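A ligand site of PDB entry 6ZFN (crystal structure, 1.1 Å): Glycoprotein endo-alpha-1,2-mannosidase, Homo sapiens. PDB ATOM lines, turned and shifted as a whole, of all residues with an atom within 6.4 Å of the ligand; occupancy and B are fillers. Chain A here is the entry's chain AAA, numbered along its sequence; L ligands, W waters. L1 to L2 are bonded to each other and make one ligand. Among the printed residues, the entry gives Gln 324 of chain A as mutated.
Water W5 lies within hydrogen-bond range of an oxygen (O3) of LG2 L2 (2.8 Å), the side-chain amide nitrogen of Asn 289 (3.1 Å) and the side-chain amide nitrogen of Asn 292 (3.3 Å).
Water W7 lies within hydrogen-bond range of OE2 of Glu 327 (2.7 Å), O1 of LG2 L2 (2.8 Å) and NH2 of Arg 286 (2.9 Å).
Water W1 bridges O of Phe 249 (2.8 Å) and O6 of LIG L1 (3.4 Å).
The side-chain carboxylate (OD2) of Asp 189 sits at hydrogen-bond distance from an oxygen (O3) of LIG L1, 2.5 Å away.
O4 of LIG L1 sits at hydrogen-bond distance from OH of Tyr 191, 2.6 Å away.
An oxygen (O2) of LG2 L2 is in hydrogen-bond range of the side-chain carboxylate (OE2) of Glu 327 (2.7 Å).
OH of Tyr 280 lies within hydrogen-bond range of O3 of LG2 L2, at 2.8 Å.
OH of Tyr 188 sits at hydrogen-bond distance from O3 of LIG L1 (2.9 Å).
An oxygen (O1) of LG2 L2 is in hydrogen-bond range of the guanidinium group (NH2) of Arg 286.
OD1 of Asp 189 sits close to OH of Tyr 191 (3.5 Å).
NH1 of Arg 286 lies within salt-bridge range of OE2 of Glu 327.
The backbone NH (N) of Glu 327 lies within hydrogen-bond range of the side-chain amide oxygen (OE1) of Gln 324, at 3.1 Å.
The side-chain hydroxyl (OH) of Tyr 280 lies within hydrogen-bond range of the guanidinium group (NH1) of Arg 286 (3.4 Å).
OH of Tyr 280 sits at hydrogen-bond distance from OD2 of Asp 282.
The side-chain carboxylate (OD2) of Asp 282 lies within salt-bridge range of the guanidinium group (NH1) of Arg 286, at 3.0 Å.
The side-chain amide nitrogen of Asn 289 lies within hydrogen-bond range of the side-chain carboxylate of Asp 282 (2.9 Å).
OD1 of Asn 289 sits at hydrogen-bond distance from ND2 of Asn 292 (2.8 Å).
Residues that only touch the ligand: Val 224 (3.6 Å), Phe 249 (3.6 Å), Trp 288 (3.7 Å), Phe 244 (3.8 Å), Thr 250 (3.8 Å), Asp 282 (3.9 Å) and Asn 289 (3.9 Å).
Within 4 Å of the ligand: Tyr 188, Asp 189, Tyr 191, Val 224, Phe 244, Phe 249, Thr 250, Tyr 280, Asp 282, Arg 286, Trp 288, Asn 289 and Glu 327.
Along chain A the residues within 4 Å of the ligand span positions 188 to 327.
The nearest printed residue that does not touch the ligand is Leu 222 (4.4 Å).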
ATOM      1  N   PRO A 145      26.221 -14.702   2.673  1.00  0.00           N
ATOM      2  CA  PRO A 145      27.510 -14.564   3.362  1.00  0.00           C
ATOM      3  C   PRO A 145      28.158 -13.247   2.950  1.00  0.00           C
ATOM      4  O   PRO A 145      28.116 -12.863   1.791  1.00  0.00           O
ATOM      5  CB  PRO A 145      28.284 -15.805   2.873  1.00  0.00           C
ATOM      6  CG  PRO A 145      27.287 -16.720   2.327  1.00  0.00           C
ATOM      7  CD  PRO A 145      26.200 -15.875   1.787  1.00  0.00           C
ATOM      8  N   TYR A 188      22.184 -17.963   5.111  1.00  0.00           N
ATOM      9  CA  TYR A 188      22.848 -18.874   4.214  1.00  0.00           C
ATOM     10  C   TYR A 188      24.271 -19.127   4.668  1.00  0.00           C
ATOM     11  O   TYR A 188      24.980 -18.195   5.029  1.00  0.00           O
ATOM     12  CB  TYR A 188      22.825 -18.360   2.768  1.00  0.00           C
ATOM     13  CG  TYR A 188      23.406 -19.329   1.774  1.00  0.00           C
ATOM     14  CD1 TYR A 188      22.674 -20.429   1.312  1.00  0.00           C
ATOM     15  CD2 TYR A 188      24.696 -19.221   1.299  1.00  0.00           C
ATOM     16  CE1 TYR A 188      23.240 -21.345   0.433  1.00  0.00           C
ATOM     17  CE2 TYR A 188      25.259 -20.094   0.435  1.00  0.00           C
ATOM     18  CZ  TYR A 188      24.535 -21.192   0.026  1.00  0.00           C
ATOM     19  OH  TYR A 188      25.079 -22.102  -0.852  1.00  0.00           O
ATOM     20  N   ASP A 189      24.712 -20.387   4.631  1.00  0.00           N
ATOM     21  CA  ASP A 189      26.075 -20.750   5.076  1.00  0.00           C
ATOM     22  C   ASP A 189      26.361 -20.217   6.471  1.00  0.00           C
ATOM     23  O   ASP A 189      27.476 -19.773   6.774  1.00  0.00           O
ATOM     24  CB  ASP A 189      27.166 -20.359   4.078  1.00  0.00           C
ATOM     25  CG  ASP A 189      27.301 -21.320   2.939  1.00  0.00           C
ATOM     26  OD1 ASP A 189      26.515 -22.304   2.890  1.00  0.00           O
ATOM     27  OD2 ASP A 189      28.191 -21.066   2.075  1.00  0.00           O
ATOM     28  N   TYR A 191      27.066 -21.788   9.005  1.00  0.00           N
ATOM     29  CA  TYR A 191      28.139 -22.505   9.687  1.00  0.00           C
ATOM     30  C   TYR A 191      29.493 -21.849   9.589  1.00  0.00           C
ATOM     31  O   TYR A 191      30.376 -22.160  10.377  1.00  0.00           O
ATOM     32  CB  TYR A 191      28.249 -23.935   9.145  1.00  0.00           C
ATOM     33  CG  TYR A 191      28.552 -24.010   7.678  1.00  0.00           C
ATOM     34  CD1 TYR A 191      29.847 -23.942   7.232  1.00  0.00           C
ATOM     35  CD2 TYR A 191      27.507 -24.074   6.713  1.00  0.00           C
ATOM     36  CE1 TYR A 191      30.148 -23.978   5.870  1.00  0.00           C
ATOM     37  CE2 TYR A 191      27.789 -24.136   5.349  1.00  0.00           C
ATOM     38  CZ  TYR A 191      29.107 -24.071   4.947  1.00  0.00           C
ATOM     39  OH  TYR A 191      29.398 -24.135   3.600  1.00  0.00           O
ATOM     40  N   LEU A 222      21.241 -22.728   7.917  1.00  0.00           N
ATOM     41  CA  LEU A 222      21.409 -23.693   6.840  1.00  0.00           C
ATOM     42  C   LEU A 222      22.108 -24.925   7.394  1.00  0.00           C
ATOM     43  O   LEU A 222      23.225 -24.827   7.923  1.00  0.00           O
ATOM     44  CB  LEU A 222      22.262 -23.117   5.721  1.00  0.00           C
ATOM     45  CG  LEU A 222      22.450 -24.063   4.543  1.00  0.00           C
ATOM     46  CD1 LEU A 222      21.142 -24.284   3.779  1.00  0.00           C
ATOM     47  CD2 LEU A 222      23.526 -23.540   3.618  1.00  0.00           C
ATOM     48  N   VAL A 224      23.965 -28.166   6.414  1.00  0.00           N
ATOM     49  CA  VAL A 224      24.644 -28.866   5.350  1.00  0.00           C
ATOM     50  C   VAL A 224      24.981 -30.286   5.758  1.00  0.00           C
ATOM     51  O   VAL A 224      24.467 -31.227   5.222  1.00  0.00           O
ATOM     52  CB  VAL A 224      25.871 -28.060   4.865  1.00  0.00           C
ATOM     53  CG1 VAL A 224      26.661 -28.817   3.817  1.00  0.00           C
ATOM     54  CG2 VAL A 224      25.428 -26.696   4.317  1.00  0.00           C
ATOM     55  N   GLU A 225      25.885 -30.401   6.753  1.00  0.00           N
ATOM     56  CA  GLU A 225      26.395 -31.694   7.235  1.00  0.00           C
ATOM     57  C   GLU A 225      25.665 -32.094   8.503  1.00  0.00           C
ATOM     58  O   GLU A 225      25.379 -31.239   9.364  1.00  0.00           O
ATOM     59  CB  GLU A 225      27.881 -31.590   7.553  1.00  0.00           C
ATOM     60  CG  GLU A 225      28.737 -31.174   6.377  1.00  0.00           C
ATOM     61  CD  GLU A 225      30.222 -30.985   6.713  1.00  0.00           C
ATOM     62  OE1 GLU A 225      30.638 -31.269   7.835  1.00  0.00           O
ATOM     63  OE2 GLU A 225      30.977 -30.533   5.844  1.00  0.00           O
ATOM     64  N   TYR A 243      18.005 -25.557   1.669  1.00  0.00           N
ATOM     65  CA  TYR A 243      18.257 -24.787   0.433  1.00  0.00           C
ATOM     66  C   TYR A 243      18.436 -25.592  -0.834  1.00  0.00           C
ATOM     67  O   TYR A 243      17.695 -25.351  -1.818  1.00  0.00           O
ATOM     68  CB  TYR A 243      19.451 -23.785   0.569  1.00  0.00           C
ATOM     69  CG  TYR A 243      19.484 -22.864  -0.629  1.00  0.00           C
ATOM     70  CD1 TYR A 243      18.606 -21.828  -0.769  1.00  0.00           C
ATOM     71  CD2 TYR A 243      20.374 -23.098  -1.662  1.00  0.00           C
ATOM     72  CE1 TYR A 243      18.544 -21.046  -1.937  1.00  0.00           C
ATOM     73  CE2 TYR A 243      20.322 -22.351  -2.838  1.00  0.00           C
ATOM     74  CZ  TYR A 243      19.413 -21.314  -2.949  1.00  0.00           C
ATOM     75  OH  TYR A 243      19.351 -20.619  -4.157  1.00  0.00           O
ATOM     76  N   PHE A 244      19.447 -26.433  -0.959  1.00  0.00           N
ATOM     77  CA  PHE A 244      19.878 -26.860  -2.268  1.00  0.00           C
ATOM     78  C   PHE A 244      18.844 -27.683  -2.970  1.00  0.00           C
ATOM     79  O   PHE A 244      18.249 -28.611  -2.413  1.00  0.00           O
ATOM     80  CB  PHE A 244      21.205 -27.649  -2.150  1.00  0.00           C
ATOM     81  CG  PHE A 244      22.267 -26.864  -1.443  1.00  0.00           C
ATOM     82  CD1 PHE A 244      22.906 -25.807  -2.073  1.00  0.00           C
ATOM     83  CD2 PHE A 244      22.556 -27.113  -0.124  1.00  0.00           C
ATOM     84  CE1 PHE A 244      23.803 -25.033  -1.380  1.00  0.00           C
ATOM     85  CE2 PHE A 244      23.472 -26.334   0.559  1.00  0.00           C
ATOM     86  CZ  PHE A 244      24.086 -25.290  -0.046  1.00  0.00           C
ATOM     87  N   PHE A 249      23.056 -33.584  -2.951  1.00  0.00           N
ATOM     88  CA  PHE A 249      24.250 -32.722  -2.892  1.00  0.00           C
ATOM     89  C   PHE A 249      24.833 -32.625  -1.481  1.00  0.00           C
ATOM     90  O   PHE A 249      26.059 -32.725  -1.331  1.00  0.00           O
ATOM     91  CB  PHE A 249      23.924 -31.347  -3.468  1.00  0.00           C
ATOM     92  CG  PHE A 249      25.015 -30.332  -3.354  1.00  0.00           C
ATOM     93  CD1 PHE A 249      26.318 -30.604  -3.758  1.00  0.00           C
ATOM     94  CD2 PHE A 249      24.778 -29.071  -2.869  1.00  0.00           C
ATOM     95  CE1 PHE A 249      27.312 -29.659  -3.676  1.00  0.00           C
ATOM     96  CE2 PHE A 249      25.767 -28.132  -2.750  1.00  0.00           C
ATOM     97  CZ  PHE A 249      27.045 -28.429  -3.143  1.00  0.00           C
ATOM     98  N   THR A 250      23.975 -32.382  -0.499  1.00  0.00           N
ATOM     99  CA  THR A 250      24.404 -32.329   0.912  1.00  0.00           C
ATOM    100  C   THR A 250      23.565 -33.303   1.713  1.00  0.00           C
ATOM    101  O   THR A 250      22.480 -33.722   1.281  1.00  0.00           O
ATOM    102  CB  THR A 250      24.259 -30.918   1.505  1.00  0.00           C
ATOM    103  OG1 THR A 250      22.875 -30.649   1.578  1.00  0.00           O
ATOM    104  CG2 THR A 250      24.989 -29.877   0.689  1.00  0.00           C
ATOM    105  N   TYR A 280      18.068 -28.785 -11.166  1.00  0.00           N
ATOM    106  CA  TYR A 280      19.298 -28.002 -10.937  1.00  0.00           C
ATOM    107  C   TYR A 280      20.160 -28.140 -12.177  1.00  0.00           C
ATOM    108  O   TYR A 280      20.356 -29.236 -12.674  1.00  0.00           O
ATOM    109  CB  TYR A 280      20.056 -28.540  -9.709  1.00  0.00           C
ATOM    110  CG  TYR A 280      21.259 -27.681  -9.358  1.00  0.00           C
ATOM    111  CD1 TYR A 280      22.493 -27.895  -9.915  1.00  0.00           C
ATOM    112  CD2 TYR A 280      21.122 -26.643  -8.452  1.00  0.00           C
ATOM    113  CE1 TYR A 280      23.580 -27.082  -9.619  1.00  0.00           C
ATOM    114  CE2 TYR A 280      22.203 -25.838  -8.142  1.00  0.00           C
ATOM    115  CZ  TYR A 280      23.400 -26.033  -8.711  1.00  0.00           C
ATOM    116  OH  TYR A 280      24.475 -25.204  -8.362  1.00  0.00           O
ATOM    117  N   ASP A 282      23.847 -25.834 -13.269  1.00  0.00           N
ATOM    118  CA  ASP A 282      24.660 -24.616 -13.185  1.00  0.00           C
ATOM    119  C   ASP A 282      25.794 -24.627 -14.153  1.00  0.00           C
ATOM    120  O   ASP A 282      26.747 -23.814 -14.034  1.00  0.00           O
ATOM    121  CB  ASP A 282      25.135 -24.346 -11.761  1.00  0.00           C
ATOM    122  CG  ASP A 282      26.127 -25.345 -11.248  1.00  0.00           C
ATOM    123  OD1 ASP A 282      26.537 -26.235 -12.018  1.00  0.00           O
ATOM    124  OD2 ASP A 282      26.481 -25.267 -10.045  1.00  0.00           O
ATOM    125  N   ARG A 286      29.459 -23.129 -14.023  1.00  0.00           N
ATOM    126  CA  ARG A 286      30.330 -24.096 -13.340  1.00  0.00           C
ATOM    127  C   ARG A 286      30.365 -25.342 -14.193  1.00  0.00           C
ATOM    128  O   ARG A 286      29.686 -26.351 -13.914  1.00  0.00           O
ATOM    129  CB  ARG A 286      29.846 -24.383 -11.946  1.00  0.00           C
ATOM    130  CG  ARG A 286      29.817 -23.174 -11.019  1.00  0.00           C
ATOM    131  CD  ARG A 286      29.331 -23.576  -9.632  1.00  0.00           C
ATOM    132  NE  ARG A 286      29.094 -22.434  -8.790  1.00  0.00           N
ATOM    133  CZ  ARG A 286      27.904 -22.012  -8.346  1.00  0.00           C
ATOM    134  NH1 ARG A 286      26.713 -22.619  -8.595  1.00  0.00           N
ATOM    135  NH2 ARG A 286      27.890 -20.923  -7.606  1.00  0.00           N
ATOM    136  N   TRP A 288      32.210 -27.790 -14.510  1.00  0.00           N
ATOM    137  CA  TRP A 288      32.691 -28.955 -13.788  1.00  0.00           C
ATOM    138  C   TRP A 288      31.688 -29.557 -12.840  1.00  0.00           C
ATOM    139  O   TRP A 288      31.991 -30.572 -12.217  1.00  0.00           O
ATOM    140  CB  TRP A 288      33.916 -28.503 -12.975  1.00  0.00           C
ATOM    141  CG  TRP A 288      33.711 -27.129 -12.238  1.00  0.00           C
ATOM    142  CD1 TRP A 288      34.008 -25.873 -12.715  1.00  0.00           C
ATOM    143  CD2 TRP A 288      33.163 -26.943 -10.949  1.00  0.00           C
ATOM    144  NE1 TRP A 288      33.662 -24.917 -11.803  1.00  0.00           N
ATOM    145  CE2 TRP A 288      33.152 -25.539 -10.703  1.00  0.00           C
ATOM    146  CE3 TRP A 288      32.683 -27.798  -9.971  1.00  0.00           C
ATOM    147  CZ2 TRP A 288      32.686 -24.998  -9.515  1.00  0.00           C
ATOM    148  CZ3 TRP A 288      32.178 -27.260  -8.808  1.00  0.00           C
ATOM    149  CH2 TRP A 288      32.199 -25.875  -8.580  1.00  0.00           C
ATOM    150  N   ASN A 289      30.497 -28.991 -12.704  1.00  0.00           N
ATOM    151  CA  ASN A 289      29.550 -29.416 -11.684  1.00  0.00           C
ATOM    152  C   ASN A 289      28.380 -30.234 -12.209  1.00  0.00           C
ATOM    153  O   ASN A 289      27.281 -30.179 -11.668  1.00  0.00           O
ATOM    154  CB  ASN A 289      29.079 -28.208 -10.871  1.00  0.00           C
ATOM    155  CG  ASN A 289      28.429 -28.573  -9.564  1.00  0.00           C
ATOM    156  OD1 ASN A 289      28.810 -29.576  -8.936  1.00  0.00           O
ATOM    157  ND2 ASN A 289      27.500 -27.748  -9.074  1.00  0.00           N
ATOM    158  N   ASN A 292      25.933 -32.618 -10.153  1.00  0.00           N
ATOM    159  CA  ASN A 292      24.818 -32.068  -9.388  1.00  0.00           C
ATOM    160  C   ASN A 292      23.648 -31.639 -10.263  1.00  0.00           C
ATOM    161  O   ASN A 292      22.613 -31.219  -9.732  1.00  0.00           O
ATOM    162  CB  ASN A 292      25.305 -30.958  -8.462  1.00  0.00           C
ATOM    163  CG  ASN A 292      26.060 -31.551  -7.292  1.00  0.00           C
ATOM    164  OD1 ASN A 292      25.502 -32.393  -6.567  1.00  0.00           O
ATOM    165  ND2 ASN A 292      27.324 -31.194  -7.121  1.00  0.00           N
ATOM    166  N   GLN A 324      16.781 -18.006  -9.417  1.00  0.00           N
ATOM    167  CA  GLN A 324      18.238 -18.249  -9.436  1.00  0.00           C
ATOM    168  C   GLN A 324      18.551 -18.918 -10.788  1.00  0.00           C
ATOM    169  O   GLN A 324      18.650 -20.131 -10.933  1.00  0.00           O
ATOM    170  CB  GLN A 324      18.716 -19.049  -8.232  1.00  0.00           C
ATOM    171  CG  GLN A 324      20.011 -18.554  -7.591  1.00  0.00           C
ATOM    172  CD  GLN A 324      21.226 -18.548  -8.465  1.00  0.00           C
ATOM    173  OE1 GLN A 324      21.129 -18.663  -9.718  1.00  0.00           O
ATOM    174  NE2 GLN A 324      22.390 -18.385  -7.866  1.00  0.00           N
ATOM    175  N   GLU A 327      21.773 -21.140 -11.507  1.00  0.00           N
ATOM    176  CA  GLU A 327      21.736 -22.500 -10.995  1.00  0.00           C
ATOM    177  C   GLU A 327      20.617 -23.333 -11.549  1.00  0.00           C
ATOM    178  O   GLU A 327      20.501 -24.510 -11.210  1.00  0.00           O
ATOM    179  CB  GLU A 327      21.705 -22.457  -9.449  1.00  0.00           C
ATOM    180  CG  GLU A 327      23.043 -21.960  -8.922  1.00  0.00           C
ATOM    181  CD  GLU A 327      23.156 -21.760  -7.432  1.00  0.00           C
ATOM    182  OE1 GLU A 327      22.097 -21.569  -6.721  1.00  0.00           O
ATOM    183  OE2 GLU A 327      24.316 -21.760  -6.967  1.00  0.00           O
HETATM  184  C1  LIG L   1      29.699 -25.182  -1.587  1.00  0.00           C
HETATM  185  C2  LIG L   1      28.998 -23.842  -1.483  1.00  0.00           C
HETATM  186  C3  LIG L   1      28.592 -23.495  -0.045  1.00  0.00           C
HETATM  187  C4  LIG L   1      27.761 -24.664   0.511  1.00  0.00           C
HETATM  188  C5  LIG L   1      28.484 -25.982   0.351  1.00  0.00           C
HETATM  189  C6  LIG L   1      27.626 -27.157   0.716  1.00  0.00           C
HETATM  190  C7  LIG L   1      31.746 -26.226  -0.896  1.00  0.00           C
HETATM  191  O1  LIG L   1      30.917 -25.056  -0.871  1.00  0.00           O
HETATM  192  O2  LIG L   1      27.782 -23.932  -2.255  1.00  0.00           O
HETATM  193  O3  LIG L   1      27.869 -22.296  -0.121  1.00  0.00           O
HETATM  194  O4  LIG L   1      27.430 -24.505   1.885  1.00  0.00           O
HETATM  195  O5  LIG L   1      28.888 -26.199  -1.009  1.00  0.00           O
HETATM  196  O6  LIG L   1      28.467 -28.347   0.763  1.00  0.00           O
HETATM  197  C1  LG2 L   2      27.805 -22.958  -3.308  1.00  0.00           C
HETATM  198  C2  LG2 L   2      26.348 -22.715  -3.733  1.00  0.00           C
HETATM  199  C3  LG2 L   2      25.768 -23.920  -4.421  1.00  0.00           C
HETATM  200  C4  LG2 L   2      26.684 -24.351  -5.538  1.00  0.00           C
HETATM  201  C5  LG2 L   2      28.061 -24.688  -4.973  1.00  0.00           C
HETATM  202  C6  LG2 L   2      29.020 -25.211  -6.051  1.00  0.00           C
HETATM  203  O1  LG2 L   2      26.325 -21.583  -4.614  1.00  0.00           O
HETATM  204  O2  LG2 L   2      24.478 -23.569  -4.919  1.00  0.00           O
HETATM  205  O3  LG2 L   2      26.106 -25.499  -6.144  1.00  0.00           O
HETATM  206  O4  LG2 L   2      28.572 -23.494  -4.385  1.00  0.00           O
HETATM  207  O5  LG2 L   2      30.252 -25.568  -5.420  1.00  0.00           O
HETATM  208  O   HOH W   1      28.391 -31.469  -0.563  1.00  0.00           O
HETATM  209  O   HOH W   2      30.558 -28.290  -4.079  1.00  0.00           O
HETATM  210  O   HOH W   3      32.861 -23.180  -1.812  1.00  0.00           O
HETATM  211  O   HOH W   4      28.635 -31.453   2.016  1.00  0.00           O
HETATM  212  O   HOH W   5      25.929 -28.256  -6.446  1.00  0.00           O
HETATM  213  O   HOH W   6      31.864 -23.788  -4.035  1.00  0.00           O
HETATM  214  O   HOH W   7      25.682 -19.500  -6.396  1.00  0.00           O
HETATM  215  O   HOH W   8      30.364 -28.475   2.484  1.00  0.00           O
